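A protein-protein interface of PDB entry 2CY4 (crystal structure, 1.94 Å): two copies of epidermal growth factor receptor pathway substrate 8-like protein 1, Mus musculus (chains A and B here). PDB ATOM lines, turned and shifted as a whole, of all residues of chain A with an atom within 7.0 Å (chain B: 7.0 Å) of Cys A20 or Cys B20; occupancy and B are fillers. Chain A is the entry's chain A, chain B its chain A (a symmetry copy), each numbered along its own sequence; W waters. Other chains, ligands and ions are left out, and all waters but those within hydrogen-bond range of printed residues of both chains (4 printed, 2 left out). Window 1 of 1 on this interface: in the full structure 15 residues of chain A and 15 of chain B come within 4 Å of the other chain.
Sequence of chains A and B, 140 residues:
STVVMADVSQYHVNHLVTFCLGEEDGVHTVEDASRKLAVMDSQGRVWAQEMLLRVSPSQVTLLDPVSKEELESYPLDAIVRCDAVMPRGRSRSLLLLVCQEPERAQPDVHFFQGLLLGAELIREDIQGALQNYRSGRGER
Of the printed residues of chain B, Cys A20 touches Cys B20 (2.2 Å), Arg B104 (3.6 Å) and Gln B106 (2.9 Å). Gly A22 touches none of the printed residues of chain B. Printed residues of chain B within 4 Å of Arg A104: Thr B18 (3.8 Å), Cys B20 (3.6 Å), Arg B104 (3.3 Å) and Asp B108 (2.9 Å). Printed residues of chain B within 4 Å of Ala A105: Thr B18 (2.9 Å) and Phe B19 (3.8 Å). Of the printed residues of chain A, Thr B18 touches Arg A104 and Ala A105. Of the printed residues of chain A, Phe B19 touches Ala A105 and Gln A106. Cys B20 touches just these residues of chain A: Cys A20, Arg A104 and Gln A106. Of the printed residues of chain A, Ala B105 touches Thr A18 (2.9 Å) and Phe A19 (3.8 Å). Val B109 touches none of the printed residues of chain A. The nearest residue of chain B that does not touch Cys A20 is Asp B108 (4.7 Å).
The backbone NH (N) of Val A109 is in hydrogen-bond range of the backbone carbonyl oxygen (O) of Phe A19 (2.8 Å). N of Val B109 sits at hydrogen-bond distance from O of Phe B19, 2.8 Å away.
Thr A18 touches Arg B104 (O to C, 3.8 Å). CB of Phe A19 touches CB of Ala B105, at 3.8 Å. OE1 of Gln B106 touches CA of Phe A19, 3.4 Å away. C of Arg A104 touches O of Thr B18 (3.8 Å). CB of Ala A105 touches CB of Phe B19 (3.8 Å). Gln A106 touches Phe B19 (OE1 to CA, 3.4 Å).
Water W1 lies within hydrogen-bond range of O of Cys A20, OD2 of Asp A25 and NE2 of Gln B106. Water W2 lies within hydrogen-bond range of O of Cys B20 (2.6 Å), OD2 of Asp B25 (3.0 Å) and NE2 of Gln A106 (3.4 Å). Water W3 bridges N of Thr B18 (2.9 Å) and N of Ala A105 (3.4 Å). Water W4 lies within hydrogen-bond range of N of Thr A18 (2.9 Å) and N of Ala B105 (3.4 Å).
The backbone carbonyl oxygen (O) of Thr A18 lies within hydrogen-bond range of the backbone NH (N) of Ala B105, 2.9 Å away. The side-chain sulfur (SG) of Cys A20 is disulfide-bonded to the side-chain sulfur (SG) of Cys B20, 2.2 Å away. The side-chain sulfur of Cys A20 is in hydrogen-bond range of the guanidinium group of Arg B104 (3.6 Å). The side-chain amide oxygen of Gln B106 is in hydrogen-bond range of the backbone NH of Cys A20 (2.9 Å). SG of Cys B20 sits at hydrogen-bond distance from NH1 of Arg A104 (3.6 Å). The side-chain carboxylate of Asp B108 lies within salt-bridge range of the guanidinium group of Arg A104 (2.9 Å). N of Ala A105 sits at hydrogen-bond distance from O of Thr B18 (2.9 Å). The backbone NH of Cys B20 lies within hydrogen-bond range of the side-chain amide oxygen of Gln A106. The guanidinium group (NH2) of Arg B104 is in salt-bridge range of the side-chain carboxylate (OD2) of Asp A108 (2.9 Å). NH2 of Arg B104 lies close to NE of Arg A104, at 3.4 Å.
Thr A18 touches Arg B104, and with the chains exchanged Arg A104 touches Thr B18. Thr A18 touches Ala B105, and with the chains exchanged Ala A105 touches Thr B18. Phe A19 touches Ala B105, and with the chains exchanged Ala A105 touches Phe B19. Arg A104 touches Asp B108, and with the chains exchanged Asp A108 touches Arg B104.
Of the 14 printed residues of chain A, 7 touch a printed residue of chain B. Hydrophobic or aromatic side chains of chain A that line the printed part of chain B: Phe A19 and Ala A105. Printed residues of chain B that touch a printed residue of chain A: Thr B18, Phe B19, Cys B20, Arg B104, Ala B105, Gln B106 and Asp B108. Hydrophobic or aromatic side chains of chain B that line the printed part of chain A: Phe B19 and Ala B105. Among the printed residues, Asp or Glu carboxylates within 4 Å of a Lys or Arg side-chain nitrogen of the other chain: Arg A104 with Asp B108 and Asp A108 with Arg B104.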
ATOM      1  N   THR A  18       7.854 -11.701 -12.235  1.00  0.00           N
ATOM      2  CA  THR A  18       9.020 -12.263 -12.919  1.00  0.00           C
ATOM      3  C   THR A  18       8.657 -12.138 -14.419  1.00  0.00           C
ATOM      4  O   THR A  18       7.566 -12.557 -14.804  1.00  0.00           O
ATOM      5  CB  THR A  18       9.312 -13.759 -12.585  1.00  0.00           C
ATOM      6  OG1 THR A  18       9.866 -13.779 -11.259  1.00  0.00           O
ATOM      7  CG2 THR A  18      10.462 -14.379 -13.611  1.00  0.00           C
ATOM      8  N   PHE A  19       9.467 -11.463 -15.260  1.00  0.00           N
ATOM      9  CA  PHE A  19       9.144 -11.487 -16.711  1.00  0.00           C
ATOM     10  C   PHE A  19      10.467 -11.594 -17.485  1.00  0.00           C
ATOM     11  O   PHE A  19      11.555 -11.227 -16.976  1.00  0.00           O
ATOM     12  CB  PHE A  19       8.339 -10.235 -17.187  1.00  0.00           C
ATOM     13  CG  PHE A  19       9.008  -8.889 -16.877  1.00  0.00           C
ATOM     14  CD1 PHE A  19      10.019  -8.394 -17.714  1.00  0.00           C
ATOM     15  CD2 PHE A  19       8.588  -8.098 -15.796  1.00  0.00           C
ATOM     16  CE1 PHE A  19      10.611  -7.150 -17.506  1.00  0.00           C
ATOM     17  CE2 PHE A  19       9.164  -6.843 -15.565  1.00  0.00           C
ATOM     18  CZ  PHE A  19      10.206  -6.363 -16.448  1.00  0.00           C
ATOM     19  N   CYS A  20      10.383 -12.113 -18.705  1.00  0.00           N
ATOM     20  CA  CYS A  20      11.574 -12.261 -19.535  1.00  0.00           C
ATOM     21  C   CYS A  20      11.908 -11.005 -20.300  1.00  0.00           C
ATOM     22  O   CYS A  20      11.021 -10.230 -20.625  1.00  0.00           O
ATOM     23  CB  CYS A  20      11.369 -13.363 -20.591  1.00  0.00           C
ATOM     24  SG  CYS A  20      10.388 -14.675 -19.850  1.00  0.00           S
ATOM     25  N   LEU A  21      13.204 -10.836 -20.566  1.00  0.00           N
ATOM     26  CA  LEU A  21      13.726  -9.789 -21.412  1.00  0.00           C
ATOM     27  C   LEU A  21      13.906 -10.470 -22.791  1.00  0.00           C
ATOM     28  O   LEU A  21      14.942 -11.104 -23.062  1.00  0.00           O
ATOM     29  CB  LEU A  21      15.084  -9.338 -20.883  1.00  0.00           C
ATOM     30  CG  LEU A  21      14.984  -8.717 -19.473  1.00  0.00           C
ATOM     31  CD1 LEU A  21      16.377  -8.376 -18.921  1.00  0.00           C
ATOM     32  CD2 LEU A  21      14.099  -7.490 -19.501  1.00  0.00           C
ATOM     33  N   GLY A  22      12.900 -10.352 -23.650  1.00  0.00           N
ATOM     34  CA  GLY A  22      13.002 -10.929 -24.975  1.00  0.00           C
ATOM     35  C   GLY A  22      13.880 -10.030 -25.788  1.00  0.00           C
ATOM     36  O   GLY A  22      14.606  -9.209 -25.237  1.00  0.00           O
ATOM     37  N   ASP A  25      10.433  -6.609 -26.885  1.00  0.00           N
ATOM     38  CA  ASP A  25       9.411  -6.293 -25.868  1.00  0.00           C
ATOM     39  C   ASP A  25       9.413  -4.788 -25.590  1.00  0.00           C
ATOM     40  O   ASP A  25       8.382  -4.177 -25.319  1.00  0.00           O
ATOM     41  CB  ASP A  25       9.734  -7.020 -24.555  1.00  0.00           C
ATOM     42  CG  ASP A  25      11.189  -6.813 -24.112  1.00  0.00           C
ATOM     43  OD1 ASP A  25      11.955  -6.073 -24.793  1.00  0.00           O
ATOM     44  OD2 ASP A  25      11.569  -7.414 -23.086  1.00  0.00           O
ATOM     45  N   VAL A  27      11.595  -3.531 -23.282  1.00  0.00           N
ATOM     46  CA  VAL A  27      12.152  -3.321 -21.938  1.00  0.00           C
ATOM     47  C   VAL A  27      13.693  -3.268 -22.018  1.00  0.00           C
ATOM     48  O   VAL A  27      14.384  -4.288 -21.978  1.00  0.00           O
ATOM     49  CB  VAL A  27      11.698  -4.407 -20.933  1.00  0.00           C
ATOM     50  CG1 VAL A  27      12.339  -4.132 -19.542  1.00  0.00           C
ATOM     51  CG2 VAL A  27      10.174  -4.333 -20.744  1.00  0.00           C
ATOM     52  N   LYS A  36       6.792  -1.409 -16.875  1.00  0.00           N
ATOM     53  CA  LYS A  36       6.098  -2.638 -17.160  1.00  0.00           C
ATOM     54  C   LYS A  36       5.438  -3.234 -15.882  1.00  0.00           C
ATOM     55  O   LYS A  36       4.370  -3.829 -15.962  1.00  0.00           O
ATOM     56  CB  LYS A  36       7.070  -3.682 -17.734  1.00  0.00           C
ATOM     57  CG  LYS A  36       6.357  -5.033 -18.026  1.00  0.00           C
ATOM     58  CD  LYS A  36       7.316  -5.950 -18.802  1.00  0.00           C
ATOM     59  CE  LYS A  36       6.776  -7.324 -18.959  1.00  0.00           C
ATOM     60  NZ  LYS A  36       5.532  -7.381 -19.786  1.00  0.00           N
ATOM     61  N   ARG A 104      17.874 -21.350 -19.871  1.00  0.00           N
ATOM     62  CA  ARG A 104      17.032 -20.390 -20.576  1.00  0.00           C
ATOM     63  C   ARG A 104      17.630 -19.613 -21.716  1.00  0.00           C
ATOM     64  O   ARG A 104      18.779 -19.244 -21.700  1.00  0.00           O
ATOM     65  CB  ARG A 104      16.406 -19.401 -19.586  1.00  0.00           C
ATOM     66  CG  ARG A 104      15.430 -20.099 -18.672  1.00  0.00           C
ATOM     67  CD  ARG A 104      14.617 -18.993 -17.945  1.00  0.00           C
ATOM     68  NE  ARG A 104      13.491 -19.642 -17.409  1.00  0.00           N
ATOM     69  CZ  ARG A 104      12.266 -19.565 -17.946  1.00  0.00           C
ATOM     70  NH1 ARG A 104      11.981 -18.814 -18.994  1.00  0.00           N
ATOM     71  NH2 ARG A 104      11.390 -20.399 -17.470  1.00  0.00           N
ATOM     72  N   ALA A 105      16.818 -19.344 -22.703  1.00  0.00           N
ATOM     73  CA  ALA A 105      17.244 -18.559 -23.853  1.00  0.00           C
ATOM     74  C   ALA A 105      17.383 -17.066 -23.514  1.00  0.00           C
ATOM     75  O   ALA A 105      18.153 -16.378 -24.114  1.00  0.00           O
ATOM     76  CB  ALA A 105      16.215 -18.715 -24.980  1.00  0.00           C
ATOM     77  N   GLN A 106      16.590 -16.546 -22.584  1.00  0.00           N
ATOM     78  CA  GLN A 106      16.637 -15.137 -22.309  1.00  0.00           C
ATOM     79  C   GLN A 106      16.809 -14.878 -20.806  1.00  0.00           C
ATOM     80  O   GLN A 106      16.552 -15.737 -19.978  1.00  0.00           O
ATOM     81  CB  GLN A 106      15.349 -14.498 -22.800  1.00  0.00           C
ATOM     82  CG  GLN A 106      14.973 -14.755 -24.312  1.00  0.00           C
ATOM     83  CD  GLN A 106      13.571 -15.474 -24.634  1.00  0.00           C
ATOM     84  OE1 GLN A 106      13.049 -16.347 -23.909  1.00  0.00           O
ATOM     85  NE2 GLN A 106      13.001 -15.108 -25.763  1.00  0.00           N
ATOM     86  N   PRO A 107      17.316 -13.704 -20.452  1.00  0.00           N
ATOM     87  CA  PRO A 107      17.465 -13.412 -19.022  1.00  0.00           C
ATOM     88  C   PRO A 107      16.069 -12.947 -18.483  1.00  0.00           C
ATOM     89  O   PRO A 107      15.118 -12.696 -19.259  1.00  0.00           O
ATOM     90  CB  PRO A 107      18.604 -12.344 -19.008  1.00  0.00           C
ATOM     91  CG  PRO A 107      18.449 -11.647 -20.323  1.00  0.00           C
ATOM     92  CD  PRO A 107      18.085 -12.757 -21.296  1.00  0.00           C
ATOM     93  N   ASP A 108      15.928 -12.896 -17.167  1.00  0.00           N
ATOM     94  CA  ASP A 108      14.653 -12.506 -16.533  1.00  0.00           C
ATOM     95  C   ASP A 108      14.818 -11.337 -15.570  1.00  0.00           C
ATOM     96  O   ASP A 108      15.841 -11.168 -14.918  1.00  0.00           O
ATOM     97  CB  ASP A 108      14.094 -13.632 -15.647  1.00  0.00           C
ATOM     98  CG  ASP A 108      13.772 -14.857 -16.413  1.00  0.00           C
ATOM     99  OD1 ASP A 108      12.952 -14.654 -17.342  1.00  0.00           O
ATOM    100  OD2 ASP A 108      14.331 -15.962 -16.083  1.00  0.00           O
ATOM    101  N   VAL A 109      13.737 -10.597 -15.420  1.00  0.00           N
ATOM    102  CA  VAL A 109      13.716  -9.522 -14.450  1.00  0.00           C
ATOM    103  C   VAL A 109      12.816  -9.950 -13.281  1.00  0.00           C
ATOM    104  O   VAL A 109      11.713 -10.470 -13.509  1.00  0.00           O
ATOM    105  CB  VAL A 109      13.063  -8.290 -15.025  1.00  0.00           C
ATOM    106  CG1 VAL A 109      12.705  -7.282 -13.865  1.00  0.00           C
ATOM    107  CG2 VAL A 109      14.005  -7.684 -16.023  1.00  0.00           C
ATOM    108  N   THR B  18      14.738 -23.514 -23.720  1.00  0.00           N
ATOM    109  CA  THR B  18      13.593 -23.022 -22.951  1.00  0.00           C
ATOM    110  C   THR B  18      13.466 -21.543 -23.393  1.00  0.00           C
ATOM    111  O   THR B  18      14.466 -20.827 -23.369  1.00  0.00           O
ATOM    112  CB  THR B  18      13.776 -23.079 -21.402  1.00  0.00           C
ATOM    113  OG1 THR B  18      13.651 -24.461 -21.028  1.00  0.00           O
ATOM    114  CG2 THR B  18      12.561 -22.247 -20.633  1.00  0.00           C
ATOM    115  N   PHE B  19      12.310 -21.089 -23.921  1.00  0.00           N
ATOM    116  CA  PHE B  19      12.196 -19.634 -24.204  1.00  0.00           C
ATOM    117  C   PHE B  19      10.771 -19.194 -23.834  1.00  0.00           C
ATOM    118  O   PHE B  19       9.823 -20.016 -23.792  1.00  0.00           O
ATOM    119  CB  PHE B  19      12.506 -19.266 -25.692  1.00  0.00           C
ATOM    120  CG  PHE B  19      11.655 -20.015 -26.726  1.00  0.00           C
ATOM    121  CD1 PHE B  19      10.357 -19.573 -27.024  1.00  0.00           C
ATOM    122  CD2 PHE B  19      12.167 -21.111 -27.437  1.00  0.00           C
ATOM    123  CE1 PHE B  19       9.571 -20.183 -27.999  1.00  0.00           C
ATOM    124  CE2 PHE B  19      11.401 -21.742 -28.424  1.00  0.00           C
ATOM    125  CZ  PHE B  19      10.065 -21.261 -28.706  1.00  0.00           C
ATOM    126  N   CYS B  20      10.620 -17.906 -23.545  1.00  0.00           N
ATOM    127  CA  CYS B  20       9.312 -17.373 -23.182  1.00  0.00           C
ATOM    128  C   CYS B  20       8.480 -17.005 -24.386  1.00  0.00           C
ATOM    129  O   CYS B  20       9.024 -16.655 -25.423  1.00  0.00           O
ATOM    130  CB  CYS B  20       9.459 -16.083 -22.354  1.00  0.00           C
ATOM    131  SG  CYS B  20      10.896 -16.263 -21.288  1.00  0.00           S
ATOM    132  N   LEU B  21       7.162 -17.100 -24.210  1.00  0.00           N
ATOM    133  CA  LEU B  21       6.184 -16.653 -25.174  1.00  0.00           C
ATOM    134  C   LEU B  21       5.781 -15.243 -24.679  1.00  0.00           C
ATOM    135  O   LEU B  21       4.893 -15.094 -23.819  1.00  0.00           O
ATOM    136  CB  LEU B  21       4.970 -17.576 -25.130  1.00  0.00           C
ATOM    137  CG  LEU B  21       5.322 -19.023 -25.539  1.00  0.00           C
ATOM    138  CD1 LEU B  21       4.110 -19.953 -25.378  1.00  0.00           C
ATOM    139  CD2 LEU B  21       5.842 -19.055 -26.961  1.00  0.00           C
ATOM    140  N   GLY B  22       6.436 -14.216 -25.207  1.00  0.00           N
ATOM    141  CA  GLY B  22       6.096 -12.860 -24.826  1.00  0.00           C
ATOM    142  C   GLY B  22       4.833 -12.497 -25.542  1.00  0.00           C
ATOM    143  O   GLY B  22       4.123 -13.373 -26.027  1.00  0.00           O
ATOM    144  N   ASP B  25       6.895 -11.387 -29.935  1.00  0.00           N
ATOM    145  CA  ASP B  25       8.060 -12.176 -30.381  1.00  0.00           C
ATOM    146  C   ASP B  25       7.780 -12.769 -31.764  1.00  0.00           C
ATOM    147  O   ASP B  25       8.668 -12.914 -32.600  1.00  0.00           O
ATOM    148  CB  ASP B  25       8.314 -13.335 -29.407  1.00  0.00           C
ATOM    149  CG  ASP B  25       7.044 -14.146 -29.117  1.00  0.00           C
ATOM    150  OD1 ASP B  25       5.960 -13.847 -29.696  1.00  0.00           O
ATOM    151  OD2 ASP B  25       7.132 -15.076 -28.289  1.00  0.00           O
ATOM    152  N   VAL B  27       6.125 -15.748 -31.984  1.00  0.00           N
ATOM    153  CA  VAL B  27       5.947 -17.199 -31.824  1.00  0.00           C
ATOM    154  C   VAL B  27       4.482 -17.503 -31.440  1.00  0.00           C
ATOM    155  O   VAL B  27       4.097 -17.482 -30.270  1.00  0.00           O
ATOM    156  CB  VAL B  27       6.917 -17.803 -30.780  1.00  0.00           C
ATOM    157  CG1 VAL B  27       6.660 -19.332 -30.652  1.00  0.00           C
ATOM    158  CG2 VAL B  27       8.368 -17.635 -31.264  1.00  0.00           C
ATOM    159  N   LYS B  36      11.924 -21.128 -34.443  1.00  0.00           N
ATOM    160  CA  LYS B  36      12.778 -20.424 -33.522  1.00  0.00           C
ATOM    161  C   LYS B  36      13.902 -21.345 -32.962  1.00  0.00           C
ATOM    162  O   LYS B  36      15.010 -20.883 -32.720  1.00  0.00           O
ATOM    163  CB  LYS B  36      11.960 -19.884 -32.337  1.00  0.00           C
ATOM    164  CG  LYS B  36      12.859 -19.141 -31.308  1.00  0.00           C
ATOM    165  CD  LYS B  36      11.964 -18.435 -30.277  1.00  0.00           C
ATOM    166  CE  LYS B  36      12.748 -17.855 -29.156  1.00  0.00           C
ATOM    167  NZ  LYS B  36      13.675 -16.765 -29.583  1.00  0.00           N
ATOM    168  N   ARG B 104       5.543 -16.564 -12.811  1.00  0.00           N
ATOM    169  CA  ARG B 104       5.890 -15.907 -14.065  1.00  0.00           C
ATOM    170  C   ARG B 104       4.822 -15.142 -14.795  1.00  0.00           C
ATOM    171  O   ARG B 104       3.672 -15.512 -14.809  1.00  0.00           O
ATOM    172  CB  ARG B 104       6.521 -16.912 -15.038  1.00  0.00           C
ATOM    173  CG  ARG B 104       7.858 -17.390 -14.527  1.00  0.00           C
ATOM    174  CD  ARG B 104       8.557 -18.127 -15.701  1.00  0.00           C
ATOM    175  NE  ARG B 104       9.910 -18.222 -15.334  1.00  0.00           N
ATOM    176  CZ  ARG B 104      10.872 -17.439 -15.840  1.00  0.00           C
ATOM    177  NH1 ARG B 104      10.654 -16.544 -16.786  1.00  0.00           N
ATOM    178  NH2 ARG B 104      12.021 -17.497 -15.235  1.00  0.00           N
ATOM    179  N   ALA B 105       5.224 -14.073 -15.429  1.00  0.00           N
ATOM    180  CA  ALA B 105       4.310 -13.259 -16.217  1.00  0.00           C
ATOM    181  C   ALA B 105       3.922 -13.942 -17.540  1.00  0.00           C
ATOM    182  O   ALA B 105       2.871 -13.708 -18.055  1.00  0.00           O
ATOM    183  CB  ALA B 105       4.975 -11.914 -16.532  1.00  0.00           C
ATOM    184  N   GLN B 106       4.802 -14.746 -18.125  1.00  0.00           N
ATOM    185  CA  GLN B 106       4.502 -15.326 -19.404  1.00  0.00           C
ATOM    186  C   GLN B 106       4.715 -16.846 -19.379  1.00  0.00           C
ATOM    187  O   GLN B 106       5.398 -17.380 -18.519  1.00  0.00           O
ATOM    188  CB  GLN B 106       5.401 -14.694 -20.452  1.00  0.00           C
ATOM    189  CG  GLN B 106       5.373 -13.118 -20.539  1.00  0.00           C
ATOM    190  CD  GLN B 106       6.752 -12.321 -20.312  1.00  0.00           C
ATOM    191  OE1 GLN B 106       7.654 -12.691 -19.531  1.00  0.00           O
ATOM    192  NE2 GLN B 106       6.867 -11.197 -20.988  1.00  0.00           N
ATOM    193  N   PRO B 107       4.068 -17.560 -20.291  1.00  0.00           N
ATOM    194  CA  PRO B 107       4.274 -19.011 -20.315  1.00  0.00           C
ATOM    195  C   PRO B 107       5.613 -19.290 -21.080  1.00  0.00           C
ATOM    196  O   PRO B 107       6.210 -18.384 -21.705  1.00  0.00           O
ATOM    197  CB  PRO B 107       2.966 -19.531 -20.993  1.00  0.00           C
ATOM    198  CG  PRO B 107       2.564 -18.404 -21.890  1.00  0.00           C
ATOM    199  CD  PRO B 107       2.885 -17.152 -21.088  1.00  0.00           C
ATOM    200  N   ASP B 108       6.112 -20.513 -20.976  1.00  0.00           N
ATOM    201  CA  ASP B 108       7.384 -20.894 -21.620  1.00  0.00           C
ATOM    202  C   ASP B 108       7.231 -22.101 -22.538  1.00  0.00           C
ATOM    203  O   ASP B 108       6.431 -22.999 -22.306  1.00  0.00           O
ATOM    204  CB  ASP B 108       8.427 -21.352 -20.588  1.00  0.00           C
ATOM    205  CG  ASP B 108       8.797 -20.282 -19.634  1.00  0.00           C
ATOM    206  OD1 ASP B 108       9.239 -19.251 -20.199  1.00  0.00           O
ATOM    207  OD2 ASP B 108       8.638 -20.485 -18.379  1.00  0.00           O
ATOM    208  N   VAL B 109       8.099 -22.147 -23.529  1.00  0.00           N
ATOM    209  CA  VAL B 109       8.143 -23.296 -24.410  1.00  0.00           C
ATOM    210  C   VAL B 109       9.417 -24.093 -24.094  1.00  0.00           C
ATOM    211  O   VAL B 109      10.498 -23.500 -23.955  1.00  0.00           O
ATOM    212  CB  VAL B 109       8.288 -22.866 -25.848  1.00  0.00           C
ATOM    213  CG1 VAL B 109       8.715 -24.099 -26.736  1.00  0.00           C
ATOM    214  CG2 VAL B 109       6.981 -22.279 -26.295  1.00  0.00           C
HETATM  215  O   HOH W   1       9.334  -9.224 -22.262  1.00  0.00           O
HETATM  216  O   HOH W   2       9.874 -14.925 -27.103  1.00  0.00           O
HETATM  217  O   HOH W   3      17.492 -22.513 -23.649  1.00  0.00           O
HETATM  218  O   HOH W   4       5.082 -12.644 -12.375  1.00  0.00           O
